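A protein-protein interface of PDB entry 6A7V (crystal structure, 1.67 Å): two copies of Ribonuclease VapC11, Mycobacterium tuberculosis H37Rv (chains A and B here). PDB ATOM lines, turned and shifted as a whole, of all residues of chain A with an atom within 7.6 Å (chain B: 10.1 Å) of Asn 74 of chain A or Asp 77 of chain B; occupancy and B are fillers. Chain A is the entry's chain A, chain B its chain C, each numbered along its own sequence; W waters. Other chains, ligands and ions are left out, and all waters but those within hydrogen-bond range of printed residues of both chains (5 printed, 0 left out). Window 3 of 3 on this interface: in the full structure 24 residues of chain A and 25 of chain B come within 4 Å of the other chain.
The side-chain carboxylate (OE1) of Glu 44 of chain A is in salt-bridge range of the guanidinium group (NE) of Arg 82 of chain B.
The backbone NH (N) of Val 75 of chain A lies within hydrogen-bond range of the side-chain carboxylate (OD2) of Asp 77 of chain B.
The side-chain carboxylate (OD1) of Asp 77 of chain A is in hydrogen-bond range of the backbone NH (N) of Val 75 of chain B (2.8 Å).
Asn 74 of chain A touches just one residue of chain B: Asp 77.
Asp 77 of chain B touches just these residues of chain A: Glu 44, Asn 74 and Val 75.
Of chain B, only Asp 77 (3.0 Å) and Phe 81 (3.97 Å) come within 4 Å of Val 75 of chain A.
Of the printed residues of chain A, Asn 74 of chain B touches Asp 77.
Of the printed residues of chain B, Asp 77 of chain A touches Asn 74 (3.6 Å) and Val 75 (2.8 Å).
Of the printed residues of chain B, Pro 45 of chain A touches Phe 81.
Of the printed residues of chain A, Phe 81 of chain B touches Glu 44, Pro 45 and Val 75.
Asp 80 of chain B touches none of the printed residues of chain A.
The nearest residue of chain B that does not touch Asn 74 of chain A is Phe 81 of chain B (7.4 Å).
The nearest residue of chain A that does not touch Asp 77 of chain B is Leu 73 of chain A (4.5 Å).
Asn 74 of chain A touches Asp 77 of chain B, and with the chains exchanged Asp 77 of chain A touches Asn 74 of chain B.
Val 75 of chain A touches Asp 77 of chain B, and with the chains exchanged Asp 77 of chain A touches Val 75 of chain B.
Positions printed for both chains: 73, 74, 75, 76, 77, 80, 109, 112 and 113.
Of the 9 pairs that touch across the chains among the printed residues, 4 have their exchanged pair printed and touching as well.
Water W5 lies within hydrogen-bond range of the backbone carbonyl oxygen of Leu 73 of chain B, the side-chain carboxylate of Asp 77 of chain A and the backbone NH of Val 75 of chain B.
Water W3 bridges OG of Ser 72 of chain A (2.7 Å) and OD2 of Asp 77 of chain B (2.8 Å).
Water W4 lies within hydrogen-bond range of OE1 of Glu 44 of chain A (2.8 Å), O of Asp 77 of chain B (2.8 Å), N of Phe 81 of chain B (3.0 Å) and N of Arg 82 of chain B (3.1 Å).
Water W2 lies within hydrogen-bond range of the backbone carbonyl oxygen of Leu 73 of chain A, the side-chain carboxylate of Asp 77 of chain B, the backbone NH of Glu 44 of chain A and the backbone NH of Val 75 of chain A.
Water W1 lies within hydrogen-bond range of the backbone carbonyl oxygen of Val 75 of chain A, the backbone NH of Asp 77 of chain B and the backbone carbonyl oxygen of Val 75 of chain B.
Of the 17 printed residues of chain A, 5 touch a printed residue of chain B.
Hydrophobic or aromatic side chains of chain A within 4 Å of the printed part of chain B: Pro 45 and Val 75.
Along chain A the printed residues that touch a printed residue of chain B span positions 44 to 77.
Among the printed residues, 9 pairs touch across the chains.
Among the printed residues, Asp or Glu carboxylates within 4 Å of a Lys or Arg side-chain nitrogen of the other chain: Glu 44 of chain A with Arg 82 of chain B.
NH2 of Arg 112 of chain A sits at hydrogen-bond distance from O of Asn 74 of chain A, at 2.8 Å.
The side-chain amide oxygen (OD1) of Asn 74 of chain A lies within hydrogen-bond range of a ring nitrogen (NE2) of His 113 of chain A, 3.0 Å away.
The backbone carbonyl oxygen (O) of Asn 74 of chain B lies within hydrogen-bond range of the guanidinium group (NH2) of Arg 112 of chain B (2.9 Å).
O of Asn 74 of chain B sits at hydrogen-bond distance from NE2 of His 113 of chain B (3.0 Å).
CG of Glu 44 of chain A touches O of Asp 77 of chain B, at 3.3 Å.
Glu 44 of chain A touches Phe 81 of chain B.
Phe 81 of chain B touches Pro 45 of chain A (CE1 to CG, 3.9 Å).
CA of Asn 74 of chain A touches OD2 of Asp 77 of chain B, at 3.4 Å.
CE2 of Phe 81 of chain B touches CG2 of Val 75 of chain A, at 3.97 Å.
Asp 77 of chain A touches Asn 74 of chain B.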
ATOM      1  N   MET A  42     -19.459  12.269 -15.499  1.00  0.00           N
ATOM      2  CA  MET A  42     -18.379  11.353 -15.796  1.00  0.00           C
ATOM      3  C   MET A  42     -18.454  10.255 -14.748  1.00  0.00           C
ATOM      4  O   MET A  42     -19.083  10.430 -13.704  1.00  0.00           O
ATOM      5  CB  MET A  42     -17.045  12.113 -15.705  1.00  0.00           C
ATOM      6  CG  MET A  42     -15.777  11.295 -15.928  1.00  0.00           C
ATOM      7  SD  MET A  42     -15.723  10.355 -17.467  1.00  0.00           S
ATOM      8  CE  MET A  42     -15.961  11.636 -18.699  1.00  0.00           C
ATOM      9  N   CYS A  43     -17.856   9.108 -15.043  1.00  0.00           N
ATOM     10  CA  CYS A  43     -17.618   8.103 -14.022  1.00  0.00           C
ATOM     11  C   CYS A  43     -16.225   7.558 -14.223  1.00  0.00           C
ATOM     12  O   CYS A  43     -15.617   7.716 -15.296  1.00  0.00           O
ATOM     13  CB  CYS A  43     -18.662   6.987 -14.049  1.00  0.00           C
ATOM     14  SG  CYS A  43     -18.637   5.902 -15.484  1.00  0.00           S
ATOM     15  N   GLU A  44     -15.711   6.911 -13.188  1.00  0.00           N
ATOM     16  CA  GLU A  44     -14.332   6.526 -13.212  1.00  0.00           C
ATOM     17  C   GLU A  44     -14.002   5.393 -14.180  1.00  0.00           C
ATOM     18  O   GLU A  44     -12.941   5.496 -14.763  1.00  0.00           O
ATOM     19  CB  GLU A  44     -13.769   6.299 -11.806  1.00  0.00           C
ATOM     20  CG  GLU A  44     -13.554   7.612 -11.067  1.00  0.00           C
ATOM     21  CD  GLU A  44     -12.481   8.480 -11.714  1.00  0.00           C
ATOM     22  OE1 GLU A  44     -11.306   8.044 -11.788  1.00  0.00           O
ATOM     23  OE2 GLU A  44     -12.812   9.602 -12.163  1.00  0.00           O
ATOM     24  N   PRO A  45     -14.923   4.480 -14.487  1.00  0.00           N
ATOM     25  CA  PRO A  45     -14.601   3.509 -15.506  1.00  0.00           C
ATOM     26  C   PRO A  45     -14.458   4.165 -16.891  1.00  0.00           C
ATOM     27  O   PRO A  45     -13.576   3.838 -17.643  1.00  0.00           O
ATOM     28  CB  PRO A  45     -15.790   2.547 -15.455  1.00  0.00           C
ATOM     29  CG  PRO A  45     -16.220   2.588 -14.033  1.00  0.00           C
ATOM     30  CD  PRO A  45     -16.001   4.015 -13.599  1.00  0.00           C
ATOM     31  N   PRO A  71     -18.766  16.491 -12.984  1.00  0.00           N
ATOM     32  CA  PRO A  71     -19.262  15.798 -11.793  1.00  0.00           C
ATOM     33  C   PRO A  71     -19.137  14.289 -11.959  1.00  0.00           C
ATOM     34  O   PRO A  71     -19.388  13.774 -13.049  1.00  0.00           O
ATOM     35  CB  PRO A  71     -20.737  16.203 -11.698  1.00  0.00           C
ATOM     36  CG  PRO A  71     -20.990  17.213 -12.761  1.00  0.00           C
ATOM     37  CD  PRO A  71     -19.748  17.428 -13.562  1.00  0.00           C
ATOM     38  N   SER A  72     -18.730  13.600 -10.895  1.00  0.00           N
ATOM     39  CA  SER A  72     -18.497  12.153 -10.943  1.00  0.00           C
ATOM     40  C   SER A  72     -19.669  11.376 -10.358  1.00  0.00           C
ATOM     41  O   SER A  72     -20.186  11.728  -9.294  1.00  0.00           O
ATOM     42  CB  SER A  72     -17.219  11.790 -10.183  1.00  0.00           C
ATOM     43  OG  SER A  72     -16.897  10.422 -10.362  1.00  0.00           O
ATOM     44  N   LEU A  73     -20.085  10.327 -11.064  1.00  0.00           N
ATOM     45  CA  LEU A  73     -21.053   9.369 -10.546  1.00  0.00           C
ATOM     46  C   LEU A  73     -20.267   8.190  -9.988  1.00  0.00           C
ATOM     47  O   LEU A  73     -19.545   7.524 -10.718  1.00  0.00           O
ATOM     48  CB  LEU A  73     -21.992   8.910 -11.656  1.00  0.00           C
ATOM     49  CG  LEU A  73     -22.768  10.021 -12.371  1.00  0.00           C
ATOM     50  CD1 LEU A  73     -23.740   9.406 -13.364  1.00  0.00           C
ATOM     51  CD2 LEU A  73     -23.507  10.914 -11.390  1.00  0.00           C
ATOM     52  N   ASN A  74     -20.394   7.943  -8.690  1.00  0.00           N
ATOM     53  CA  ASN A  74     -19.494   7.016  -8.015  1.00  0.00           C
ATOM     54  C   ASN A  74     -19.688   5.552  -8.416  1.00  0.00           C
ATOM     55  O   ASN A  74     -20.776   5.140  -8.815  1.00  0.00           O
ATOM     56  CB  ASN A  74     -19.631   7.144  -6.493  1.00  0.00           C
ATOM     57  CG  ASN A  74     -20.859   6.434  -5.953  1.00  0.00           C
ATOM     58  OD1 ASN A  74     -21.955   6.593  -6.476  1.00  0.00           O
ATOM     59  ND2 ASN A  74     -20.674   5.633  -4.908  1.00  0.00           N
ATOM     60  N   VAL A  75     -18.605   4.790  -8.317  1.00  0.00           N
ATOM     61  CA  VAL A  75     -18.673   3.338  -8.327  1.00  0.00           C
ATOM     62  C   VAL A  75     -18.875   2.901  -6.879  1.00  0.00           C
ATOM     63  O   VAL A  75     -18.070   3.243  -6.004  1.00  0.00           O
ATOM     64  CB  VAL A  75     -17.373   2.712  -8.861  1.00  0.00           C
ATOM     65  CG1 VAL A  75     -17.412   1.190  -8.726  1.00  0.00           C
ATOM     66  CG2 VAL A  75     -17.134   3.110 -10.315  1.00  0.00           C
ATOM     67  N   ASP A  76     -19.956   2.167  -6.633  1.00  0.00           N
ATOM     68  CA  ASP A  76     -20.218   1.565  -5.339  1.00  0.00           C
ATOM     69  C   ASP A  76     -19.659   0.150  -5.400  1.00  0.00           C
ATOM     70  O   ASP A  76     -20.240  -0.741  -6.025  1.00  0.00           O
ATOM     71  CB  ASP A  76     -21.720   1.555  -5.032  1.00  0.00           C
ATOM     72  CG  ASP A  76     -22.031   1.087  -3.616  1.00  0.00           C
ATOM     73  OD1 ASP A  76     -21.307   0.219  -3.079  1.00  0.00           O
ATOM     74  OD2 ASP A  76     -23.013   1.590  -3.038  1.00  0.00           O
ATOM     75  N   ASP A  77     -18.512  -0.026  -4.753  1.00  0.00           N
ATOM     76  CA  ASP A  77     -17.769  -1.281  -4.717  1.00  0.00           C
ATOM     77  C   ASP A  77     -18.631  -2.497  -4.359  1.00  0.00           C
ATOM     78  O   ASP A  77     -18.491  -3.563  -4.953  1.00  0.00           O
ATOM     79  CB  ASP A  77     -16.633  -1.125  -3.692  1.00  0.00           C
ATOM     80  CG  ASP A  77     -15.899  -2.408  -3.425  1.00  0.00           C
ATOM     81  OD1 ASP A  77     -14.972  -2.735  -4.185  1.00  0.00           O
ATOM     82  OD2 ASP A  77     -16.238  -3.081  -2.435  1.00  0.00           O
ATOM     83  N   ASP A  80     -21.901  -2.619  -7.539  1.00  0.00           N
ATOM     84  CA  ASP A  80     -21.905  -2.304  -8.965  1.00  0.00           C
ATOM     85  C   ASP A  80     -21.279  -3.464  -9.760  1.00  0.00           C
ATOM     86  O   ASP A  80     -21.831  -3.849 -10.780  1.00  0.00           O
ATOM     87  CB  ASP A  80     -21.229  -0.968  -9.285  1.00  0.00           C
ATOM     88  CG  ASP A  80     -22.086   0.242  -8.916  1.00  0.00           C
ATOM     89  OD1 ASP A  80     -23.328   0.121  -8.758  1.00  0.00           O
ATOM     90  OD2 ASP A  80     -21.506   1.343  -8.796  1.00  0.00           O
ATOM     91  N   ALA A 108     -24.568  -0.584 -15.133  1.00  0.00           N
ATOM     92  CA  ALA A 108     -25.008  -0.756 -13.752  1.00  0.00           C
ATOM     93  C   ALA A 108     -24.964   0.559 -13.015  1.00  0.00           C
ATOM     94  O   ALA A 108     -25.898   0.900 -12.268  1.00  0.00           O
ATOM     95  CB  ALA A 108     -24.159  -1.803 -13.038  1.00  0.00           C
ATOM     96  N   LEU A 109     -23.835   1.264 -13.186  1.00  0.00           N
ATOM     97  CA  LEU A 109     -23.609   2.552 -12.548  1.00  0.00           C
ATOM     98  C   LEU A 109     -24.735   3.532 -12.937  1.00  0.00           C
ATOM     99  O   LEU A 109     -25.333   4.233 -12.103  1.00  0.00           O
ATOM    100  CB  LEU A 109     -22.202   3.041 -12.923  1.00  0.00           C
ATOM    101  CG  LEU A 109     -21.609   4.264 -12.255  1.00  0.00           C
ATOM    102  CD1 LEU A 109     -20.099   4.106 -12.152  1.00  0.00           C
ATOM    103  CD2 LEU A 109     -21.975   5.509 -13.043  1.00  0.00           C
ATOM    104  N   ALA A 110     -25.003   3.531 -14.229  1.00  0.00           N
ATOM    105  CA  ALA A 110     -25.997   4.440 -14.815  1.00  0.00           C
ATOM    106  C   ALA A 110     -27.374   4.159 -14.256  1.00  0.00           C
ATOM    107  O   ALA A 110     -28.097   5.059 -13.898  1.00  0.00           O
ATOM    108  CB  ALA A 110     -25.987   4.344 -16.330  1.00  0.00           C
ATOM    109  N   ARG A 112     -28.033   2.708 -11.426  1.00  0.00           N
ATOM    110  CA  ARG A 112     -28.090   3.033 -10.004  1.00  0.00           C
ATOM    111  C   ARG A 112     -28.274   4.534  -9.841  1.00  0.00           C
ATOM    112  O   ARG A 112     -29.039   4.950  -8.956  1.00  0.00           O
ATOM    113  CB  ARG A 112     -26.898   2.520  -9.211  1.00  0.00           C
ATOM    114  CG  ARG A 112     -27.094   2.674  -7.708  1.00  0.00           C
ATOM    115  CD  ARG A 112     -26.027   1.938  -6.918  1.00  0.00           C
ATOM    116  NE  ARG A 112     -24.697   2.255  -7.423  1.00  0.00           N
ATOM    117  CZ  ARG A 112     -24.051   3.396  -7.204  1.00  0.00           C
ATOM    118  NH1 ARG A 112     -24.586   4.362  -6.463  1.00  0.00           N
ATOM    119  NH2 ARG A 112     -22.849   3.575  -7.732  1.00  0.00           N
ATOM    120  N   HIS A 113     -27.592   5.346 -10.651  1.00  0.00           N
ATOM    121  CA  HIS A 113     -27.679   6.771 -10.502  1.00  0.00           C
ATOM    122  C   HIS A 113     -28.921   7.380 -11.136  1.00  0.00           C
ATOM    123  O   HIS A 113     -29.158   8.538 -10.948  1.00  0.00           O
ATOM    124  CB  HIS A 113     -26.405   7.420 -11.054  1.00  0.00           C
ATOM    125  CG  HIS A 113     -25.226   7.288 -10.139  1.00  0.00           C
ATOM    126  ND1 HIS A 113     -25.023   8.135  -9.071  1.00  0.00           N
ATOM    127  CD2 HIS A 113     -24.198   6.406 -10.122  1.00  0.00           C
ATOM    128  CE1 HIS A 113     -23.916   7.784  -8.439  1.00  0.00           C
ATOM    129  NE2 HIS A 113     -23.396   6.738  -9.056  1.00  0.00           N
ATOM    130  N   LEU B  73     -10.863  -6.797  -0.692  1.00  0.00           N
ATOM    131  CA  LEU B  73     -10.060  -5.595  -0.872  1.00  0.00           C
ATOM    132  C   LEU B  73     -10.849  -4.659  -1.781  1.00  0.00           C
ATOM    133  O   LEU B  73     -11.107  -4.992  -2.930  1.00  0.00           O
ATOM    134  CB  LEU B  73      -8.714  -5.947  -1.501  1.00  0.00           C
ATOM    135  CG  LEU B  73      -7.898  -7.038  -0.793  1.00  0.00           C
ATOM    136  CD1 LEU B  73      -6.578  -7.255  -1.511  1.00  0.00           C
ATOM    137  CD2 LEU B  73      -7.666  -6.697   0.666  1.00  0.00           C
ATOM    138  N   ASN B  74     -11.237  -3.494  -1.266  1.00  0.00           N
ATOM    139  CA  ASN B  74     -12.162  -2.621  -1.994  1.00  0.00           C
ATOM    140  C   ASN B  74     -11.531  -1.938  -3.203  1.00  0.00           C
ATOM    141  O   ASN B  74     -10.306  -1.804  -3.307  1.00  0.00           O
ATOM    142  CB  ASN B  74     -12.806  -1.582  -1.053  1.00  0.00           C
ATOM    143  CG  ASN B  74     -11.870  -0.440  -0.675  1.00  0.00           C
ATOM    144  OD1 ASN B  74     -10.647  -0.556  -0.739  1.00  0.00           O
ATOM    145  ND2 ASN B  74     -12.459   0.678  -0.269  1.00  0.00           N
ATOM    146  N   VAL B  75     -12.394  -1.546  -4.131  1.00  0.00           N
ATOM    147  CA  VAL B  75     -12.058  -0.599  -5.169  1.00  0.00           C
ATOM    148  C   VAL B  75     -12.467   0.769  -4.639  1.00  0.00           C
ATOM    149  O   VAL B  75     -13.609   0.959  -4.210  1.00  0.00           O
ATOM    150  CB  VAL B  75     -12.834  -0.880  -6.470  1.00  0.00           C
ATOM    151  CG1 VAL B  75     -12.582   0.224  -7.493  1.00  0.00           C
ATOM    152  CG2 VAL B  75     -12.458  -2.243  -7.032  1.00  0.00           C
ATOM    153  N   ASP B  76     -11.527   1.705  -4.657  1.00  0.00           N
ATOM    154  CA  ASP B  76     -11.773   3.078  -4.237  1.00  0.00           C
ATOM    155  C   ASP B  76     -11.661   3.939  -5.479  1.00  0.00           C
ATOM    156  O   ASP B  76     -10.563   4.132  -6.002  1.00  0.00           O
ATOM    157  CB  ASP B  76     -10.731   3.501  -3.193  1.00  0.00           C
ATOM    158  CG  ASP B  76     -10.984   4.898  -2.637  1.00  0.00           C
ATOM    159  OD1 ASP B  76     -11.603   5.728  -3.337  1.00  0.00           O
ATOM    160  OD2 ASP B  76     -10.559   5.167  -1.494  1.00  0.00           O
ATOM    161  N   ASP B  77     -12.791   4.448  -5.974  1.00  0.00           N
ATOM    162  CA  ASP B  77     -12.762   5.178  -7.241  1.00  0.00           C
ATOM    163  C   ASP B  77     -12.155   6.586  -7.140  1.00  0.00           C
ATOM    164  O   ASP B  77     -11.978   7.246  -8.146  1.00  0.00           O
ATOM    165  CB  ASP B  77     -14.132   5.173  -7.940  1.00  0.00           C
ATOM    166  CG  ASP B  77     -15.127   6.124  -7.322  1.00  0.00           C
ATOM    167  OD1 ASP B  77     -14.914   6.589  -6.185  1.00  0.00           O
ATOM    168  OD2 ASP B  77     -16.143   6.404  -7.998  1.00  0.00           O
ATOM    169  N   ALA B  78     -11.785   7.026  -5.938  1.00  0.00           N
ATOM    170  CA  ALA B  78     -10.969   8.237  -5.810  1.00  0.00           C
ATOM    171  C   ALA B  78      -9.505   7.983  -6.205  1.00  0.00           C
ATOM    172  O   ALA B  78      -8.727   8.929  -6.316  1.00  0.00           O
ATOM    173  CB  ALA B  78     -11.035   8.765  -4.385  1.00  0.00           C
ATOM    174  N   ILE B  79      -9.132   6.714  -6.399  1.00  0.00           N
ATOM    175  CA  ILE B  79      -7.737   6.327  -6.593  1.00  0.00           C
ATOM    176  C   ILE B  79      -7.479   5.312  -7.719  1.00  0.00           C
ATOM    177  O   ILE B  79      -6.599   5.521  -8.558  1.00  0.00           O
ATOM    178  CB  ILE B  79      -7.171   5.699  -5.298  1.00  0.00           C
ATOM    179  CG1 ILE B  79      -7.470   6.582  -4.076  1.00  0.00           C
ATOM    180  CG2 ILE B  79      -5.671   5.459  -5.440  1.00  0.00           C
ATOM    181  CD1 ILE B  79      -7.132   5.922  -2.752  1.00  0.00           C
ATOM    182  N   ASP B  80      -8.224   4.209  -7.724  1.00  0.00           N
ATOM    183  CA  ASP B  80      -7.782   3.000  -8.373  1.00  0.00           C
ATOM    184  C   ASP B  80      -7.954   3.067  -9.878  1.00  0.00           C
ATOM    185  O   ASP B  80      -7.089   2.516 -10.566  1.00  0.00           O
ATOM    186  CB  ASP B  80      -8.498   1.770  -7.819  1.00  0.00           C
ATOM    187  CG  ASP B  80      -8.150   1.493  -6.370  1.00  0.00           C
ATOM    188  OD1 ASP B  80      -7.040   1.881  -5.922  1.00  0.00           O
ATOM    189  OD2 ASP B  80      -9.000   0.889  -5.676  1.00  0.00           O
ATOM    190  N   PHE B  81      -8.988   3.727 -10.388  1.00  0.00           N
ATOM    191  CA  PHE B  81      -9.170   3.785 -11.818  1.00  0.00           C
ATOM    192  C   PHE B  81      -8.074   4.608 -12.501  1.00  0.00           C
ATOM    193  O   PHE B  81      -7.515   4.167 -13.514  1.00  0.00           O
ATOM    194  CB  PHE B  81     -10.580   4.253 -12.177  1.00  0.00           C
ATOM    195  CG  PHE B  81     -11.637   3.253 -11.813  1.00  0.00           C
ATOM    196  CD1 PHE B  81     -11.965   2.218 -12.688  1.00  0.00           C
ATOM    197  CD2 PHE B  81     -12.273   3.310 -10.588  1.00  0.00           C
ATOM    198  CE1 PHE B  81     -12.927   1.278 -12.346  1.00  0.00           C
ATOM    199  CE2 PHE B  81     -13.235   2.374 -10.240  1.00  0.00           C
ATOM    200  CZ  PHE B  81     -13.563   1.360 -11.123  1.00  0.00           C
ATOM    201  N   ARG B  82      -7.734   5.748 -11.875  1.00  0.00           N
ATOM    202  CA  ARG B  82      -6.644   6.568 -12.366  1.00  0.00           C
ATOM    203  C   ARG B  82      -5.331   5.779 -12.346  1.00  0.00           C
ATOM    204  O   ARG B  82      -4.567   5.845 -13.318  1.00  0.00           O
ATOM    205  CB  ARG B  82      -6.486   7.878 -11.568  1.00  0.00           C
ATOM    206  CG  ARG B  82      -7.689   8.817 -11.589  1.00  0.00           C
ATOM    207  CD  ARG B  82      -8.255   9.075 -12.986  1.00  0.00           C
ATOM    208  NE  ARG B  82      -9.496   9.833 -12.868  1.00  0.00           N
ATOM    209  CZ  ARG B  82      -9.577  11.158 -12.774  1.00  0.00           C
ATOM    210  NH1 ARG B  82     -10.761  11.728 -12.618  1.00  0.00           N
ATOM    211  NH2 ARG B  82      -8.490  11.922 -12.840  1.00  0.00           N
ATOM    212  N   ALA B  83      -5.108   5.023 -11.270  1.00  0.00           N
ATOM    213  CA  ALA B  83      -3.900   4.231 -11.169  1.00  0.00           C
ATOM    214  C   ALA B  83      -3.832   3.177 -12.281  1.00  0.00           C
ATOM    215  O   ALA B  83      -2.779   2.997 -12.901  1.00  0.00           O
ATOM    216  CB  ALA B  83      -3.773   3.597  -9.783  1.00  0.00           C
ATOM    217  N   ALA B  84      -4.962   2.551 -12.557  1.00  0.00           N
ATOM    218  CA  ALA B  84      -5.056   1.573 -13.625  1.00  0.00           C
ATOM    219  C   ALA B  84      -4.710   2.184 -14.959  1.00  0.00           C
ATOM    220  O   ALA B  84      -3.945   1.587 -15.746  1.00  0.00           O
ATOM    221  CB  ALA B  84      -6.443   0.956 -13.661  1.00  0.00           C
ATOM    222  N   LEU B 105      -6.441  -2.646 -13.303  1.00  0.00           N
ATOM    223  CA  LEU B 105      -7.233  -2.277 -12.174  1.00  0.00           C
ATOM    224  C   LEU B 105      -6.935  -3.159 -10.962  1.00  0.00           C
ATOM    225  O   LEU B 105      -6.710  -2.637  -9.833  1.00  0.00           O
ATOM    226  CB  LEU B 105      -8.732  -2.325 -12.489  1.00  0.00           C
ATOM    227  CG  LEU B 105      -9.684  -1.887 -11.363  1.00  0.00           C
ATOM    228  CD1 LEU B 105      -9.427  -0.457 -10.908  1.00  0.00           C
ATOM    229  CD2 LEU B 105     -11.128  -2.044 -11.826  1.00  0.00           C
ATOM    230  N   LEU B 109      -5.215  -2.151  -7.405  1.00  0.00           N
ATOM    231  CA  LEU B 109      -5.823  -2.318  -6.092  1.00  0.00           C
ATOM    232  C   LEU B 109      -4.900  -3.169  -5.205  1.00  0.00           C
ATOM    233  O   LEU B 109      -4.759  -2.851  -4.019  1.00  0.00           O
ATOM    234  CB  LEU B 109      -7.287  -2.743  -6.141  1.00  0.00           C
ATOM    235  CG  LEU B 109      -7.664  -4.158  -6.505  1.00  0.00           C
ATOM    236  CD1 LEU B 109      -7.617  -5.062  -5.283  1.00  0.00           C
ATOM    237  CD2 LEU B 109      -9.059  -4.146  -7.118  1.00  0.00           C
ATOM    238  N   ARG B 112      -2.224  -0.949  -3.886  1.00  0.00           N
ATOM    239  CA  ARG B 112      -2.724  -0.051  -2.861  1.00  0.00           C
ATOM    240  C   ARG B 112      -2.844  -0.815  -1.556  1.00  0.00           C
ATOM    241  O   ARG B 112      -2.494  -0.250  -0.483  1.00  0.00           O
ATOM    242  CB  ARG B 112      -4.023   0.623  -3.238  1.00  0.00           C
ATOM    243  CG  ARG B 112      -4.493   1.574  -2.156  1.00  0.00           C
ATOM    244  CD  ARG B 112      -5.589   2.489  -2.643  1.00  0.00           C
ATOM    245  NE  ARG B 112      -6.752   1.748  -3.115  1.00  0.00           N
ATOM    246  CZ  ARG B 112      -7.697   1.214  -2.341  1.00  0.00           C
ATOM    247  NH1 ARG B 112      -7.630   1.282  -1.016  1.00  0.00           N
ATOM    248  NH2 ARG B 112      -8.722   0.576  -2.908  1.00  0.00           N
ATOM    249  N   HIS B 113      -3.332  -2.053  -1.608  1.00  0.00           N
ATOM    250  CA  HIS B 113      -3.657  -2.764  -0.383  1.00  0.00           C
ATOM    251  C   HIS B 113      -2.497  -3.524   0.228  1.00  0.00           C
ATOM    252  O   HIS B 113      -2.623  -4.123   1.279  1.00  0.00           O
ATOM    253  CB  HIS B 113      -4.820  -3.741  -0.658  1.00  0.00           C
ATOM    254  CG  HIS B 113      -6.160  -3.082  -0.766  1.00  0.00           C
ATOM    255  ND1 HIS B 113      -6.877  -2.674   0.337  1.00  0.00           N
ATOM    256  CD2 HIS B 113      -6.941  -2.813  -1.840  1.00  0.00           C
ATOM    257  CE1 HIS B 113      -8.028  -2.159  -0.052  1.00  0.00           C
ATOM    258  NE2 HIS B 113      -8.092  -2.232  -1.369  1.00  0.00           N
HETATM  259  O   HOH W   1     -15.276   3.046  -5.618  1.00  0.00           O
HETATM  260  O   HOH W   2     -16.894   6.745 -10.661  1.00  0.00           O
HETATM  261  O   HOH W   3     -16.753   9.178  -7.961  1.00  0.00           O
HETATM  262  O   HOH W   4      -9.947   6.548  -9.921  1.00  0.00           O
HETATM  263  O   HOH W   5     -13.276  -4.812  -4.477  1.00  0.00           O
